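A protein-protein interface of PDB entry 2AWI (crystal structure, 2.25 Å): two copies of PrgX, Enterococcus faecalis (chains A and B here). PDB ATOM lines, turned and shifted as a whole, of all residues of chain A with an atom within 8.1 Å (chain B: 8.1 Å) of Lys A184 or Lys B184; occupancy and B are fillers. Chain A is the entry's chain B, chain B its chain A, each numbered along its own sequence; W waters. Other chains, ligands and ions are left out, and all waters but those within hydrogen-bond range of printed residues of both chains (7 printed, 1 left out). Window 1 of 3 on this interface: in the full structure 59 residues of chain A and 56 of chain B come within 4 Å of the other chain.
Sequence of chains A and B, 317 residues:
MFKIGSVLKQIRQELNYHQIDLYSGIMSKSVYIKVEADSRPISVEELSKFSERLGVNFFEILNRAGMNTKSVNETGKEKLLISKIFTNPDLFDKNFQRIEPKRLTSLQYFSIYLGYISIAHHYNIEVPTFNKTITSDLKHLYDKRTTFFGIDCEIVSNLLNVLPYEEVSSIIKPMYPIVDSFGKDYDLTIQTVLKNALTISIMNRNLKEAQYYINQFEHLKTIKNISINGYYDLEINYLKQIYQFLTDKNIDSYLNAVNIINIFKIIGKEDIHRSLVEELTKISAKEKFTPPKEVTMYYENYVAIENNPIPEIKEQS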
ATOM      1  N   PHE A  59      30.180  28.748 -10.319  1.00  0.00           N
ATOM      2  CA  PHE A  59      29.625  28.251  -9.066  1.00  0.00           C
ATOM      3  C   PHE A  59      30.674  27.773  -8.077  1.00  0.00           C
ATOM      4  O   PHE A  59      30.480  27.885  -6.863  1.00  0.00           O
ATOM      5  CB  PHE A  59      28.605  27.132  -9.324  1.00  0.00           C
ATOM      6  CG  PHE A  59      27.289  27.622  -9.876  1.00  0.00           C
ATOM      7  CD1 PHE A  59      26.956  27.417 -11.210  1.00  0.00           C
ATOM      8  CD2 PHE A  59      26.387  28.299  -9.058  1.00  0.00           C
ATOM      9  CE1 PHE A  59      25.742  27.878 -11.727  1.00  0.00           C
ATOM     10  CE2 PHE A  59      25.169  28.766  -9.565  1.00  0.00           C
ATOM     11  CZ  PHE A  59      24.850  28.554 -10.904  1.00  0.00           C
ATOM     12  N   ASN A  63      31.241  29.140  -4.170  1.00  0.00           N
ATOM     13  CA  ASN A  63      31.343  28.285  -3.002  1.00  0.00           C
ATOM     14  C   ASN A  63      32.690  28.432  -2.311  1.00  0.00           C
ATOM     15  O   ASN A  63      32.784  28.287  -1.092  1.00  0.00           O
ATOM     16  CB  ASN A  63      31.102  26.827  -3.374  1.00  0.00           C
ATOM     17  CG  ASN A  63      29.630  26.488  -3.434  1.00  0.00           C
ATOM     18  OD1 ASN A  63      28.873  26.840  -2.532  1.00  0.00           O
ATOM     19  ND2 ASN A  63      29.215  25.796  -4.489  1.00  0.00           N
ATOM     20  N   SER A 181      15.474  21.771 -16.114  1.00  0.00           N
ATOM     21  CA  SER A 181      16.394  21.522 -15.026  1.00  0.00           C
ATOM     22  C   SER A 181      17.003  22.867 -14.682  1.00  0.00           C
ATOM     23  O   SER A 181      17.384  23.617 -15.576  1.00  0.00           O
ATOM     24  CB  SER A 181      17.495  20.552 -15.477  1.00  0.00           C
ATOM     25  OG  SER A 181      18.444  20.321 -14.439  1.00  0.00           O
ATOM     26  N   PHE A 182      17.081  23.190 -13.397  1.00  0.00           N
ATOM     27  CA  PHE A 182      17.666  24.458 -12.993  1.00  0.00           C
ATOM     28  C   PHE A 182      18.841  24.287 -12.041  1.00  0.00           C
ATOM     29  O   PHE A 182      18.959  24.991 -11.041  1.00  0.00           O
ATOM     30  CB  PHE A 182      16.585  25.367 -12.396  1.00  0.00           C
ATOM     31  CG  PHE A 182      15.565  25.814 -13.407  1.00  0.00           C
ATOM     32  CD1 PHE A 182      15.966  26.511 -14.547  1.00  0.00           C
ATOM     33  CD2 PHE A 182      14.217  25.502 -13.248  1.00  0.00           C
ATOM     34  CE1 PHE A 182      15.036  26.890 -15.521  1.00  0.00           C
ATOM     35  CE2 PHE A 182      13.276  25.875 -14.215  1.00  0.00           C
ATOM     36  CZ  PHE A 182      13.688  26.573 -15.359  1.00  0.00           C
ATOM     37  N   GLY A 183      19.720  23.347 -12.377  1.00  0.00           N
ATOM     38  CA  GLY A 183      20.892  23.103 -11.552  1.00  0.00           C
ATOM     39  C   GLY A 183      20.791  21.843 -10.716  1.00  0.00           C
ATOM     40  O   GLY A 183      19.692  21.389 -10.390  1.00  0.00           O
ATOM     41  N   LYS A 184      21.944  21.290 -10.352  1.00  0.00           N
ATOM     42  CA  LYS A 184      21.997  20.060  -9.567  1.00  0.00           C
ATOM     43  C   LYS A 184      21.282  20.135  -8.225  1.00  0.00           C
ATOM     44  O   LYS A 184      20.662  19.161  -7.792  1.00  0.00           O
ATOM     45  CB  LYS A 184      23.450  19.624  -9.366  1.00  0.00           C
ATOM     46  CG  LYS A 184      24.139  19.150 -10.645  1.00  0.00           C
ATOM     47  CD  LYS A 184      25.521  18.584 -10.344  1.00  0.00           C
ATOM     48  CE  LYS A 184      26.185  17.988 -11.590  1.00  0.00           C
ATOM     49  NZ  LYS A 184      26.502  19.014 -12.635  1.00  0.00           N
ATOM     50  N   ASP A 185      21.365  21.282  -7.561  1.00  0.00           N
ATOM     51  CA  ASP A 185      20.699  21.459  -6.270  1.00  0.00           C
ATOM     52  C   ASP A 185      19.199  21.287  -6.470  1.00  0.00           C
ATOM     53  O   ASP A 185      18.549  20.505  -5.785  1.00  0.00           O
ATOM     54  CB  ASP A 185      21.014  22.848  -5.704  1.00  0.00           C
ATOM     55  CG  ASP A 185      22.390  22.919  -5.048  1.00  0.00           C
ATOM     56  OD1 ASP A 185      22.845  24.038  -4.722  1.00  0.00           O
ATOM     57  OD2 ASP A 185      23.013  21.851  -4.843  1.00  0.00           O
ATOM     58  N   TYR A 186      18.663  22.014  -7.440  1.00  0.00           N
ATOM     59  CA  TYR A 186      17.251  21.948  -7.783  1.00  0.00           C
ATOM     60  C   TYR A 186      16.873  20.519  -8.187  1.00  0.00           C
ATOM     61  O   TYR A 186      15.845  19.991  -7.740  1.00  0.00           O
ATOM     62  CB  TYR A 186      16.979  22.941  -8.922  1.00  0.00           C
ATOM     63  CG  TYR A 186      15.634  22.820  -9.588  1.00  0.00           C
ATOM     64  CD1 TYR A 186      15.429  21.908 -10.628  1.00  0.00           C
ATOM     65  CD2 TYR A 186      14.563  23.635  -9.196  1.00  0.00           C
ATOM     66  CE1 TYR A 186      14.191  21.813 -11.263  1.00  0.00           C
ATOM     67  CE2 TYR A 186      13.331  23.549  -9.818  1.00  0.00           C
ATOM     68  CZ  TYR A 186      13.148  22.637 -10.852  1.00  0.00           C
ATOM     69  OH  TYR A 186      11.925  22.548 -11.467  1.00  0.00           O
ATOM     70  N   ASP A 187      17.712  19.896  -9.017  1.00  0.00           N
ATOM     71  CA  ASP A 187      17.465  18.531  -9.480  1.00  0.00           C
ATOM     72  C   ASP A 187      17.222  17.569  -8.323  1.00  0.00           C
ATOM     73  O   ASP A 187      16.306  16.749  -8.366  1.00  0.00           O
ATOM     74  CB  ASP A 187      18.645  18.013 -10.320  1.00  0.00           C
ATOM     75  CG  ASP A 187      18.713  18.641 -11.715  1.00  0.00           C
ATOM     76  OD1 ASP A 187      19.706  18.373 -12.430  1.00  0.00           O
ATOM     77  OD2 ASP A 187      17.783  19.394 -12.101  1.00  0.00           O
ATOM     78  N   LEU A 188      18.044  17.667  -7.285  1.00  0.00           N
ATOM     79  CA  LEU A 188      17.917  16.793  -6.124  1.00  0.00           C
ATOM     80  C   LEU A 188      16.561  16.971  -5.452  1.00  0.00           C
ATOM     81  O   LEU A 188      15.821  16.010  -5.235  1.00  0.00           O
ATOM     82  CB  LEU A 188      19.009  17.116  -5.095  1.00  0.00           C
ATOM     83  CG  LEU A 188      19.692  15.974  -4.323  1.00  0.00           C
ATOM     84  CD1 LEU A 188      20.125  16.485  -2.955  1.00  0.00           C
ATOM     85  CD2 LEU A 188      18.771  14.786  -4.166  1.00  0.00           C
ATOM     86  N   THR A 189      16.252  18.217  -5.117  1.00  0.00           N
ATOM     87  CA  THR A 189      15.017  18.557  -4.434  1.00  0.00           C
ATOM     88  C   THR A 189      13.755  18.054  -5.125  1.00  0.00           C
ATOM     89  O   THR A 189      12.835  17.590  -4.456  1.00  0.00           O
ATOM     90  CB  THR A 189      14.917  20.071  -4.255  1.00  0.00           C
ATOM     91  OG1 THR A 189      16.103  20.544  -3.601  1.00  0.00           O
ATOM     92  CG2 THR A 189      13.689  20.434  -3.433  1.00  0.00           C
ATOM     93  N   ILE A 190      13.711  18.133  -6.453  1.00  0.00           N
ATOM     94  CA  ILE A 190      12.533  17.680  -7.181  1.00  0.00           C
ATOM     95  C   ILE A 190      12.416  16.157  -7.230  1.00  0.00           C
ATOM     96  O   ILE A 190      11.338  15.622  -7.493  1.00  0.00           O
ATOM     97  CB  ILE A 190      12.499  18.247  -8.624  1.00  0.00           C
ATOM     98  CG1 ILE A 190      13.702  17.746  -9.417  1.00  0.00           C
ATOM     99  CG2 ILE A 190      12.488  19.777  -8.578  1.00  0.00           C
ATOM    100  CD1 ILE A 190      13.734  18.224 -10.837  1.00  0.00           C
ATOM    101  N   GLN A 191      13.516  15.461  -6.967  1.00  0.00           N
ATOM    102  CA  GLN A 191      13.515  14.000  -6.953  1.00  0.00           C
ATOM    103  C   GLN A 191      13.136  13.493  -5.571  1.00  0.00           C
ATOM    104  O   GLN A 191      12.457  12.477  -5.434  1.00  0.00           O
ATOM    105  CB  GLN A 191      14.892  13.456  -7.322  1.00  0.00           C
ATOM    106  CG  GLN A 191      15.250  13.630  -8.784  1.00  0.00           C
ATOM    107  CD  GLN A 191      16.692  13.277  -9.066  1.00  0.00           C
ATOM    108  OE1 GLN A 191      17.514  14.152  -9.344  1.00  0.00           O
ATOM    109  NE2 GLN A 191      17.011  11.993  -8.986  1.00  0.00           N
ATOM    110  N   ASN A 225      19.970  18.028 -19.484  1.00  0.00           N
ATOM    111  CA  ASN A 225      20.908  18.434 -18.439  1.00  0.00           C
ATOM    112  C   ASN A 225      20.501  18.022 -17.033  1.00  0.00           C
ATOM    113  O   ASN A 225      21.073  18.492 -16.057  1.00  0.00           O
ATOM    114  CB  ASN A 225      21.121  19.951 -18.458  1.00  0.00           C
ATOM    115  CG  ASN A 225      21.759  20.439 -19.744  1.00  0.00           C
ATOM    116  OD1 ASN A 225      22.622  19.774 -20.321  1.00  0.00           O
ATOM    117  ND2 ASN A 225      21.349  21.620 -20.192  1.00  0.00           N
ATOM    118  N   ILE A 226      19.511  17.148 -16.926  1.00  0.00           N
ATOM    119  CA  ILE A 226      19.047  16.698 -15.623  1.00  0.00           C
ATOM    120  C   ILE A 226      20.128  15.856 -14.938  1.00  0.00           C
ATOM    121  O   ILE A 226      20.912  15.177 -15.599  1.00  0.00           O
ATOM    122  CB  ILE A 226      17.756  15.844 -15.764  1.00  0.00           C
ATOM    123  CG1 ILE A 226      17.156  15.554 -14.393  1.00  0.00           C
ATOM    124  CG2 ILE A 226      18.071  14.512 -16.444  1.00  0.00           C
ATOM    125  CD1 ILE A 226      16.551  16.750 -13.739  1.00  0.00           C
ATOM    126  N   SER A 227      20.169  15.907 -13.612  1.00  0.00           N
ATOM    127  CA  SER A 227      21.126  15.119 -12.847  1.00  0.00           C
ATOM    128  C   SER A 227      20.356  14.160 -11.960  1.00  0.00           C
ATOM    129  O   SER A 227      20.008  14.495 -10.836  1.00  0.00           O
ATOM    130  CB  SER A 227      22.009  16.008 -11.968  1.00  0.00           C
ATOM    131  OG  SER A 227      22.907  16.772 -12.750  1.00  0.00           O
ATOM    132  N   ILE A 228      20.093  12.964 -12.466  1.00  0.00           N
ATOM    133  CA  ILE A 228      19.367  11.972 -11.693  1.00  0.00           C
ATOM    134  C   ILE A 228      20.273  11.435 -10.593  1.00  0.00           C
ATOM    135  O   ILE A 228      21.455  11.169 -10.823  1.00  0.00           O
ATOM    136  CB  ILE A 228      18.910  10.793 -12.584  1.00  0.00           C
ATOM    137  CG1 ILE A 228      18.041  11.309 -13.738  1.00  0.00           C
ATOM    138  CG2 ILE A 228      18.161   9.767 -11.745  1.00  0.00           C
ATOM    139  CD1 ILE A 228      16.681  11.869 -13.295  1.00  0.00           C
ATOM    140  N   ASN A 229      19.703  11.280  -9.401  1.00  0.00           N
ATOM    141  CA  ASN A 229      20.412  10.765  -8.239  1.00  0.00           C
ATOM    142  C   ASN A 229      20.388   9.239  -8.259  1.00  0.00           C
ATOM    143  O   ASN A 229      19.334   8.611  -8.076  1.00  0.00           O
ATOM    144  CB  ASN A 229      19.753  11.289  -6.955  1.00  0.00           C
ATOM    145  CG  ASN A 229      20.333  10.668  -5.705  1.00  0.00           C
ATOM    146  OD1 ASN A 229      20.353   9.444  -5.561  1.00  0.00           O
ATOM    147  ND2 ASN A 229      20.802  11.505  -4.788  1.00  0.00           N
ATOM    148  N   PHE B  59      21.062  29.789  -6.112  1.00  0.00           N
ATOM    149  CA  PHE B  59      21.544  29.096  -7.306  1.00  0.00           C
ATOM    150  C   PHE B  59      20.426  28.853  -8.317  1.00  0.00           C
ATOM    151  O   PHE B  59      20.640  28.954  -9.525  1.00  0.00           O
ATOM    152  CB  PHE B  59      22.191  27.751  -6.939  1.00  0.00           C
ATOM    153  CG  PHE B  59      23.561  27.867  -6.308  1.00  0.00           C
ATOM    154  CD1 PHE B  59      24.217  26.731  -5.848  1.00  0.00           C
ATOM    155  CD2 PHE B  59      24.190  29.097  -6.159  1.00  0.00           C
ATOM    156  CE1 PHE B  59      25.477  26.819  -5.248  1.00  0.00           C
ATOM    157  CE2 PHE B  59      25.449  29.193  -5.560  1.00  0.00           C
ATOM    158  CZ  PHE B  59      26.089  28.055  -5.104  1.00  0.00           C
ATOM    159  N   ASN B  63      20.490  29.966 -12.201  1.00  0.00           N
ATOM    160  CA  ASN B  63      20.217  29.028 -13.279  1.00  0.00           C
ATOM    161  C   ASN B  63      19.034  29.496 -14.115  1.00  0.00           C
ATOM    162  O   ASN B  63      19.114  29.525 -15.338  1.00  0.00           O
ATOM    163  CB  ASN B  63      19.944  27.630 -12.717  1.00  0.00           C
ATOM    164  CG  ASN B  63      21.216  26.861 -12.416  1.00  0.00           C
ATOM    165  OD1 ASN B  63      21.863  26.342 -13.317  1.00  0.00           O
ATOM    166  ND2 ASN B  63      21.583  26.791 -11.143  1.00  0.00           N
ATOM    167  N   SER B 181      34.518  20.095  -0.051  1.00  0.00           N
ATOM    168  CA  SER B 181      33.520  19.976  -1.111  1.00  0.00           C
ATOM    169  C   SER B 181      33.141  21.385  -1.510  1.00  0.00           C
ATOM    170  O   SER B 181      32.903  22.218  -0.648  1.00  0.00           O
ATOM    171  CB  SER B 181      32.262  19.268  -0.614  1.00  0.00           C
ATOM    172  OG  SER B 181      31.171  19.541  -1.483  1.00  0.00           O
ATOM    173  N   PHE B 182      33.079  21.657  -2.806  1.00  0.00           N
ATOM    174  CA  PHE B 182      32.723  22.993  -3.268  1.00  0.00           C
ATOM    175  C   PHE B 182      31.514  23.014  -4.201  1.00  0.00           C
ATOM    176  O   PHE B 182      31.511  23.730  -5.202  1.00  0.00           O
ATOM    177  CB  PHE B 182      33.931  23.647  -3.949  1.00  0.00           C
ATOM    178  CG  PHE B 182      35.044  23.990  -2.999  1.00  0.00           C
ATOM    179  CD1 PHE B 182      34.815  24.842  -1.921  1.00  0.00           C
ATOM    180  CD2 PHE B 182      36.317  23.458  -3.170  1.00  0.00           C
ATOM    181  CE1 PHE B 182      35.840  25.158  -1.026  1.00  0.00           C
ATOM    182  CE2 PHE B 182      37.348  23.770  -2.280  1.00  0.00           C
ATOM    183  CZ  PHE B 182      37.109  24.619  -1.208  1.00  0.00           C
ATOM    184  N   GLY B 183      30.482  22.243  -3.858  1.00  0.00           N
ATOM    185  CA  GLY B 183      29.290  22.195  -4.688  1.00  0.00           C
ATOM    186  C   GLY B 183      29.128  20.874  -5.427  1.00  0.00           C
ATOM    187  O   GLY B 183      30.097  20.135  -5.617  1.00  0.00           O
ATOM    188  N   LYS B 184      27.901  20.583  -5.854  1.00  0.00           N
ATOM    189  CA  LYS B 184      27.604  19.351  -6.572  1.00  0.00           C
ATOM    190  C   LYS B 184      28.350  19.228  -7.902  1.00  0.00           C
ATOM    191  O   LYS B 184      28.789  18.143  -8.260  1.00  0.00           O
ATOM    192  CB  LYS B 184      26.095  19.227  -6.788  1.00  0.00           C
ATOM    193  CG  LYS B 184      25.322  18.984  -5.495  1.00  0.00           C
ATOM    194  CD  LYS B 184      23.858  18.666  -5.772  1.00  0.00           C
ATOM    195  CE  LYS B 184      23.126  18.303  -4.495  1.00  0.00           C
ATOM    196  NZ  LYS B 184      23.106  19.440  -3.511  1.00  0.00           N
ATOM    197  N   ASP B 185      28.499  20.327  -8.635  1.00  0.00           N
ATOM    198  CA  ASP B 185      29.221  20.288  -9.906  1.00  0.00           C
ATOM    199  C   ASP B 185      30.663  19.850  -9.655  1.00  0.00           C
ATOM    200  O   ASP B 185      31.175  18.946 -10.318  1.00  0.00           O
ATOM    201  CB  ASP B 185      29.228  21.668 -10.564  1.00  0.00           C
ATOM    202  CG  ASP B 185      27.854  22.090 -11.058  1.00  0.00           C
ATOM    203  OD1 ASP B 185      27.672  23.297 -11.344  1.00  0.00           O
ATOM    204  OD2 ASP B 185      26.970  21.216 -11.171  1.00  0.00           O
ATOM    205  N   TYR B 186      31.299  20.494  -8.681  1.00  0.00           N
ATOM    206  CA  TYR B 186      32.679  20.200  -8.313  1.00  0.00           C
ATOM    207  C   TYR B 186      32.793  18.743  -7.850  1.00  0.00           C
ATOM    208  O   TYR B 186      33.688  18.013  -8.283  1.00  0.00           O
ATOM    209  CB  TYR B 186      33.121  21.183  -7.216  1.00  0.00           C
ATOM    210  CG  TYR B 186      34.427  20.855  -6.535  1.00  0.00           C
ATOM    211  CD1 TYR B 186      34.457  20.086  -5.370  1.00  0.00           C
ATOM    212  CD2 TYR B 186      35.637  21.312  -7.058  1.00  0.00           C
ATOM    213  CE1 TYR B 186      35.667  19.782  -4.741  1.00  0.00           C
ATOM    214  CE2 TYR B 186      36.840  21.015  -6.442  1.00  0.00           C
ATOM    215  CZ  TYR B 186      36.854  20.251  -5.289  1.00  0.00           C
ATOM    216  OH  TYR B 186      38.061  19.945  -4.701  1.00  0.00           O
ATOM    217  N   ASP B 187      31.867  18.322  -6.992  1.00  0.00           N
ATOM    218  CA  ASP B 187      31.847  16.953  -6.486  1.00  0.00           C
ATOM    219  C   ASP B 187      31.850  15.911  -7.611  1.00  0.00           C
ATOM    220  O   ASP B 187      32.603  14.936  -7.562  1.00  0.00           O
ATOM    221  CB  ASP B 187      30.607  16.725  -5.619  1.00  0.00           C
ATOM    222  CG  ASP B 187      30.651  17.493  -4.307  1.00  0.00           C
ATOM    223  OD1 ASP B 187      29.699  17.348  -3.518  1.00  0.00           O
ATOM    224  OD2 ASP B 187      31.627  18.234  -4.059  1.00  0.00           O
ATOM    225  N   LEU B 188      31.006  16.117  -8.619  1.00  0.00           N
ATOM    226  CA  LEU B 188      30.896  15.181  -9.732  1.00  0.00           C
ATOM    227  C   LEU B 188      32.221  15.056 -10.478  1.00  0.00           C
ATOM    228  O   LEU B 188      32.691  13.959 -10.762  1.00  0.00           O
ATOM    229  CB  LEU B 188      29.819  15.652 -10.711  1.00  0.00           C
ATOM    230  CG  LEU B 188      29.055  14.623 -11.555  1.00  0.00           C
ATOM    231  CD1 LEU B 188      28.681  15.268 -12.867  1.00  0.00           C
ATOM    232  CD2 LEU B 188      29.876  13.389 -11.812  1.00  0.00           C
ATOM    233  N   THR B 189      32.810  16.199 -10.787  1.00  0.00           N
ATOM    234  CA  THR B 189      34.063  16.264 -11.515  1.00  0.00           C
ATOM    235  C   THR B 189      35.238  15.571 -10.824  1.00  0.00           C
ATOM    236  O   THR B 189      36.013  14.866 -11.466  1.00  0.00           O
ATOM    237  CB  THR B 189      34.428  17.716 -11.776  1.00  0.00           C
ATOM    238  OG1 THR B 189      33.312  18.369 -12.396  1.00  0.00           O
ATOM    239  CG2 THR B 189      35.642  17.803 -12.689  1.00  0.00           C
ATOM    240  N   ILE B 190      35.373  15.767  -9.520  1.00  0.00           N
ATOM    241  CA  ILE B 190      36.465  15.142  -8.799  1.00  0.00           C
ATOM    242  C   ILE B 190      36.256  13.633  -8.706  1.00  0.00           C
ATOM    243  O   ILE B 190      37.212  12.884  -8.498  1.00  0.00           O
ATOM    244  CB  ILE B 190      36.603  15.734  -7.387  1.00  0.00           C
ATOM    245  CG1 ILE B 190      35.361  15.403  -6.560  1.00  0.00           C
ATOM    246  CG2 ILE B 190      36.781  17.249  -7.481  1.00  0.00           C
ATOM    247  CD1 ILE B 190      35.439  15.894  -5.141  1.00  0.00           C
ATOM    248  N   GLN B 191      35.005  13.195  -8.873  1.00  0.00           N
ATOM    249  CA  GLN B 191      34.658  11.776  -8.815  1.00  0.00           C
ATOM    250  C   GLN B 191      34.874  11.076 -10.148  1.00  0.00           C
ATOM    251  O   GLN B 191      35.297   9.924 -10.190  1.00  0.00           O
ATOM    252  CB  GLN B 191      33.196  11.599  -8.403  1.00  0.00           C
ATOM    253  CG  GLN B 191      32.959  11.520  -6.907  1.00  0.00           C
ATOM    254  CD  GLN B 191      31.488  11.638  -6.547  1.00  0.00           C
ATOM    255  OE1 GLN B 191      30.950  12.740  -6.447  1.00  0.00           O
ATOM    256  NE2 GLN B 191      30.829  10.500  -6.366  1.00  0.00           N
ATOM    257  N   ASN B 225      29.328  17.550   3.712  1.00  0.00           N
ATOM    258  CA  ASN B 225      28.433  18.014   2.650  1.00  0.00           C
ATOM    259  C   ASN B 225      28.792  17.547   1.239  1.00  0.00           C
ATOM    260  O   ASN B 225      28.446  18.212   0.260  1.00  0.00           O
ATOM    261  CB  ASN B 225      28.345  19.545   2.654  1.00  0.00           C
ATOM    262  CG  ASN B 225      27.703  20.093   3.921  1.00  0.00           C
ATOM    263  OD1 ASN B 225      26.716  19.545   4.420  1.00  0.00           O
ATOM    264  ND2 ASN B 225      28.250  21.189   4.433  1.00  0.00           N
ATOM    265  N   ILE B 226      29.477  16.412   1.131  1.00  0.00           N
ATOM    266  CA  ILE B 226      29.867  15.880  -0.174  1.00  0.00           C
ATOM    267  C   ILE B 226      28.664  15.218  -0.849  1.00  0.00           C
ATOM    268  O   ILE B 226      27.792  14.671  -0.180  1.00  0.00           O
ATOM    269  CB  ILE B 226      30.987  14.811  -0.038  1.00  0.00           C
ATOM    270  CG1 ILE B 226      31.558  14.464  -1.413  1.00  0.00           C
ATOM    271  CG2 ILE B 226      30.427  13.541   0.608  1.00  0.00           C
ATOM    272  CD1 ILE B 226      32.304  15.592  -2.052  1.00  0.00           C
ATOM    273  N   SER B 227      28.619  15.267  -2.172  1.00  0.00           N
ATOM    274  CA  SER B 227      27.533  14.639  -2.914  1.00  0.00           C
ATOM    275  C   SER B 227      28.078  13.485  -3.738  1.00  0.00           C
ATOM    276  O   SER B 227      28.450  13.661  -4.899  1.00  0.00           O
ATOM    277  CB  SER B 227      26.858  15.639  -3.851  1.00  0.00           C
ATOM    278  OG  SER B 227      25.978  16.486  -3.141  1.00  0.00           O
ATOM    279  N   ILE B 228      28.137  12.305  -3.136  1.00  0.00           N
ATOM    280  CA  ILE B 228      28.634  11.134  -3.844  1.00  0.00           C
ATOM    281  C   ILE B 228      27.617  10.743  -4.923  1.00  0.00           C
ATOM    282  O   ILE B 228      26.413  10.732  -4.676  1.00  0.00           O
ATOM    283  CB  ILE B 228      28.833   9.930  -2.874  1.00  0.00           C
ATOM    284  CG1 ILE B 228      29.775  10.321  -1.726  1.00  0.00           C
ATOM    285  CG2 ILE B 228      29.384   8.733  -3.640  1.00  0.00           C
ATOM    286  CD1 ILE B 228      31.217  10.631  -2.186  1.00  0.00           C
ATOM    287  N   ASN B 229      28.108  10.430  -6.115  1.00  0.00           N
ATOM    288  CA  ASN B 229      27.256  10.029  -7.223  1.00  0.00           C
ATOM    289  C   ASN B 229      26.923   8.557  -7.051  1.00  0.00           C
ATOM    290  O   ASN B 229      27.815   7.703  -7.070  1.00  0.00           O
ATOM    291  CB  ASN B 229      27.990  10.249  -8.547  1.00  0.00           C
ATOM    292  CG  ASN B 229      27.198   9.771  -9.754  1.00  0.00           C
ATOM    293  OD1 ASN B 229      26.862   8.592  -9.873  1.00  0.00           O
ATOM    294  ND2 ASN B 229      26.904  10.691 -10.661  1.00  0.00           N
HETATM  295  O   HOH W   1      29.633  18.672 -12.894  1.00  0.00           O
HETATM  296  O   HOH W   2      23.818  11.277 -11.802  1.00  0.00           O
HETATM  297  O   HOH W   3      23.908  11.402  -3.814  1.00  0.00           O
HETATM  298  O   HOH W   4      23.534  10.762  -6.582  1.00  0.00           O
HETATM  299  O   HOH W   5      25.750  22.178  -4.650  1.00  0.00           O
HETATM  300  O   HOH W   6      24.038  10.120  -9.363  1.00  0.00           O
HETATM  301  O   HOH W   7      24.391  22.660 -11.574  1.00  0.00           O
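Lys B184 touches just these residues of chain A: Lys A184 (3.7 Å), Asp A185 (2.8 Å) and Leu A188 (3.8 Å).
Of the printed residues of chain B, Gly A183 touches Asn B63.
Gly B183 touches just one residue of chain A: Asn A63.
Printed residues of chain B within 4 Å of Asp A185: Phe B59 and Lys B184.
Printed residues of chain B within 4 Å of Phe A182: Asn B63 (3.2 Å).
Of the printed residues of chain B, Leu A188 touches Lys B184.
The nearest printed residue of chain A that does not touch Phe B182 is Phe A59 (4.6 Å).
Phe B59 touches Phe A59.
Asn B63 touches Phe A59.
Phe B59 touches Asn A63.
Gly B183 touches Asn A63 (CA to ND2, 3.6 Å).
Asn B63 touches Gly A183 (ND2 to CA, 3.8 Å).
CD of Lys A184 touches CB of Lys B184 (3.7 Å).
Leu B188 touches Lys A184 (CD1 to CE, 3.9 Å).
Asp A185 touches Phe B59.
CD1 of Leu A188 touches CE of Lys B184, 3.8 Å away.
The backbone carbonyl oxygen (O) of Phe A59 is in hydrogen-bond range of the side-chain amide nitrogen (ND2) of Asn A63 (3.4 Å).
The side-chain hydroxyl (OG1) of Thr A189 sits at hydrogen-bond distance from the backbone carbonyl oxygen (O) of Asp A185.
The backbone carbonyl oxygen (O) of Asp B185 sits at hydrogen-bond distance from the side-chain hydroxyl (OG1) of Thr B189 (3.0 Å).
Water W2 lies within hydrogen-bond range of the backbone carbonyl oxygen (O) of Ile A228 and the side-chain amide nitrogen (ND2) of Asn B229.
Water W3 bridges O of Ile B228 (2.7 Å) and ND2 of Asn A229 (3.3 Å).
Water W1 bridges the backbone carbonyl oxygen (O) of Asp B185 and the side-chain amino group (NZ) of Lys A184.
The side-chain carboxylate (OD2) of Asp A185 is in salt-bridge range of the side-chain amino group (NZ) of Lys B184, 2.8 Å away.
ND2 of Asn A63 sits at hydrogen-bond distance from O of Phe B182, at 3.2 Å.
The side-chain amide nitrogen of Asn B63 lies within hydrogen-bond range of the backbone carbonyl oxygen of Phe A182 (3.2 Å).
The side-chain carboxylate (OD2) of Asp B185 is in salt-bridge range of the side-chain amino group (NZ) of Lys A184, at 2.7 Å.
Along chain A the printed residues that touch a printed residue of chain B span positions 59 to 188.
Of the 18 printed residues of chain B, 7 touch a printed residue of chain A.
Hydrophobic or aromatic side chains of chain B that line the printed part of chain A: Phe B59 and Leu B188.
Among the printed residues, 13 pairs touch across the chains.
Among the printed residues, Asp or Glu carboxylates within 4 Å of a Lys or Arg side-chain nitrogen of the other chain: Lys A184 with Asp B185 and Asp A185 with Lys B184.
Asn A63 touches Gly B183, and with the chains exchanged Gly A183 touches Asn B63.
Lys A184 touches Leu B188, and with the chains exchanged Leu A188 touches Lys B184.
Positions printed for both chains: 59, 63, 181, 182, 183, 184, 185, 186, 187, 188, 189, 190, 191, 225, 226, 227, 228 and 229.
Of the 13 pairs that touch across the chains among the printed residues, 12 have their exchanged pair printed and touching as well.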
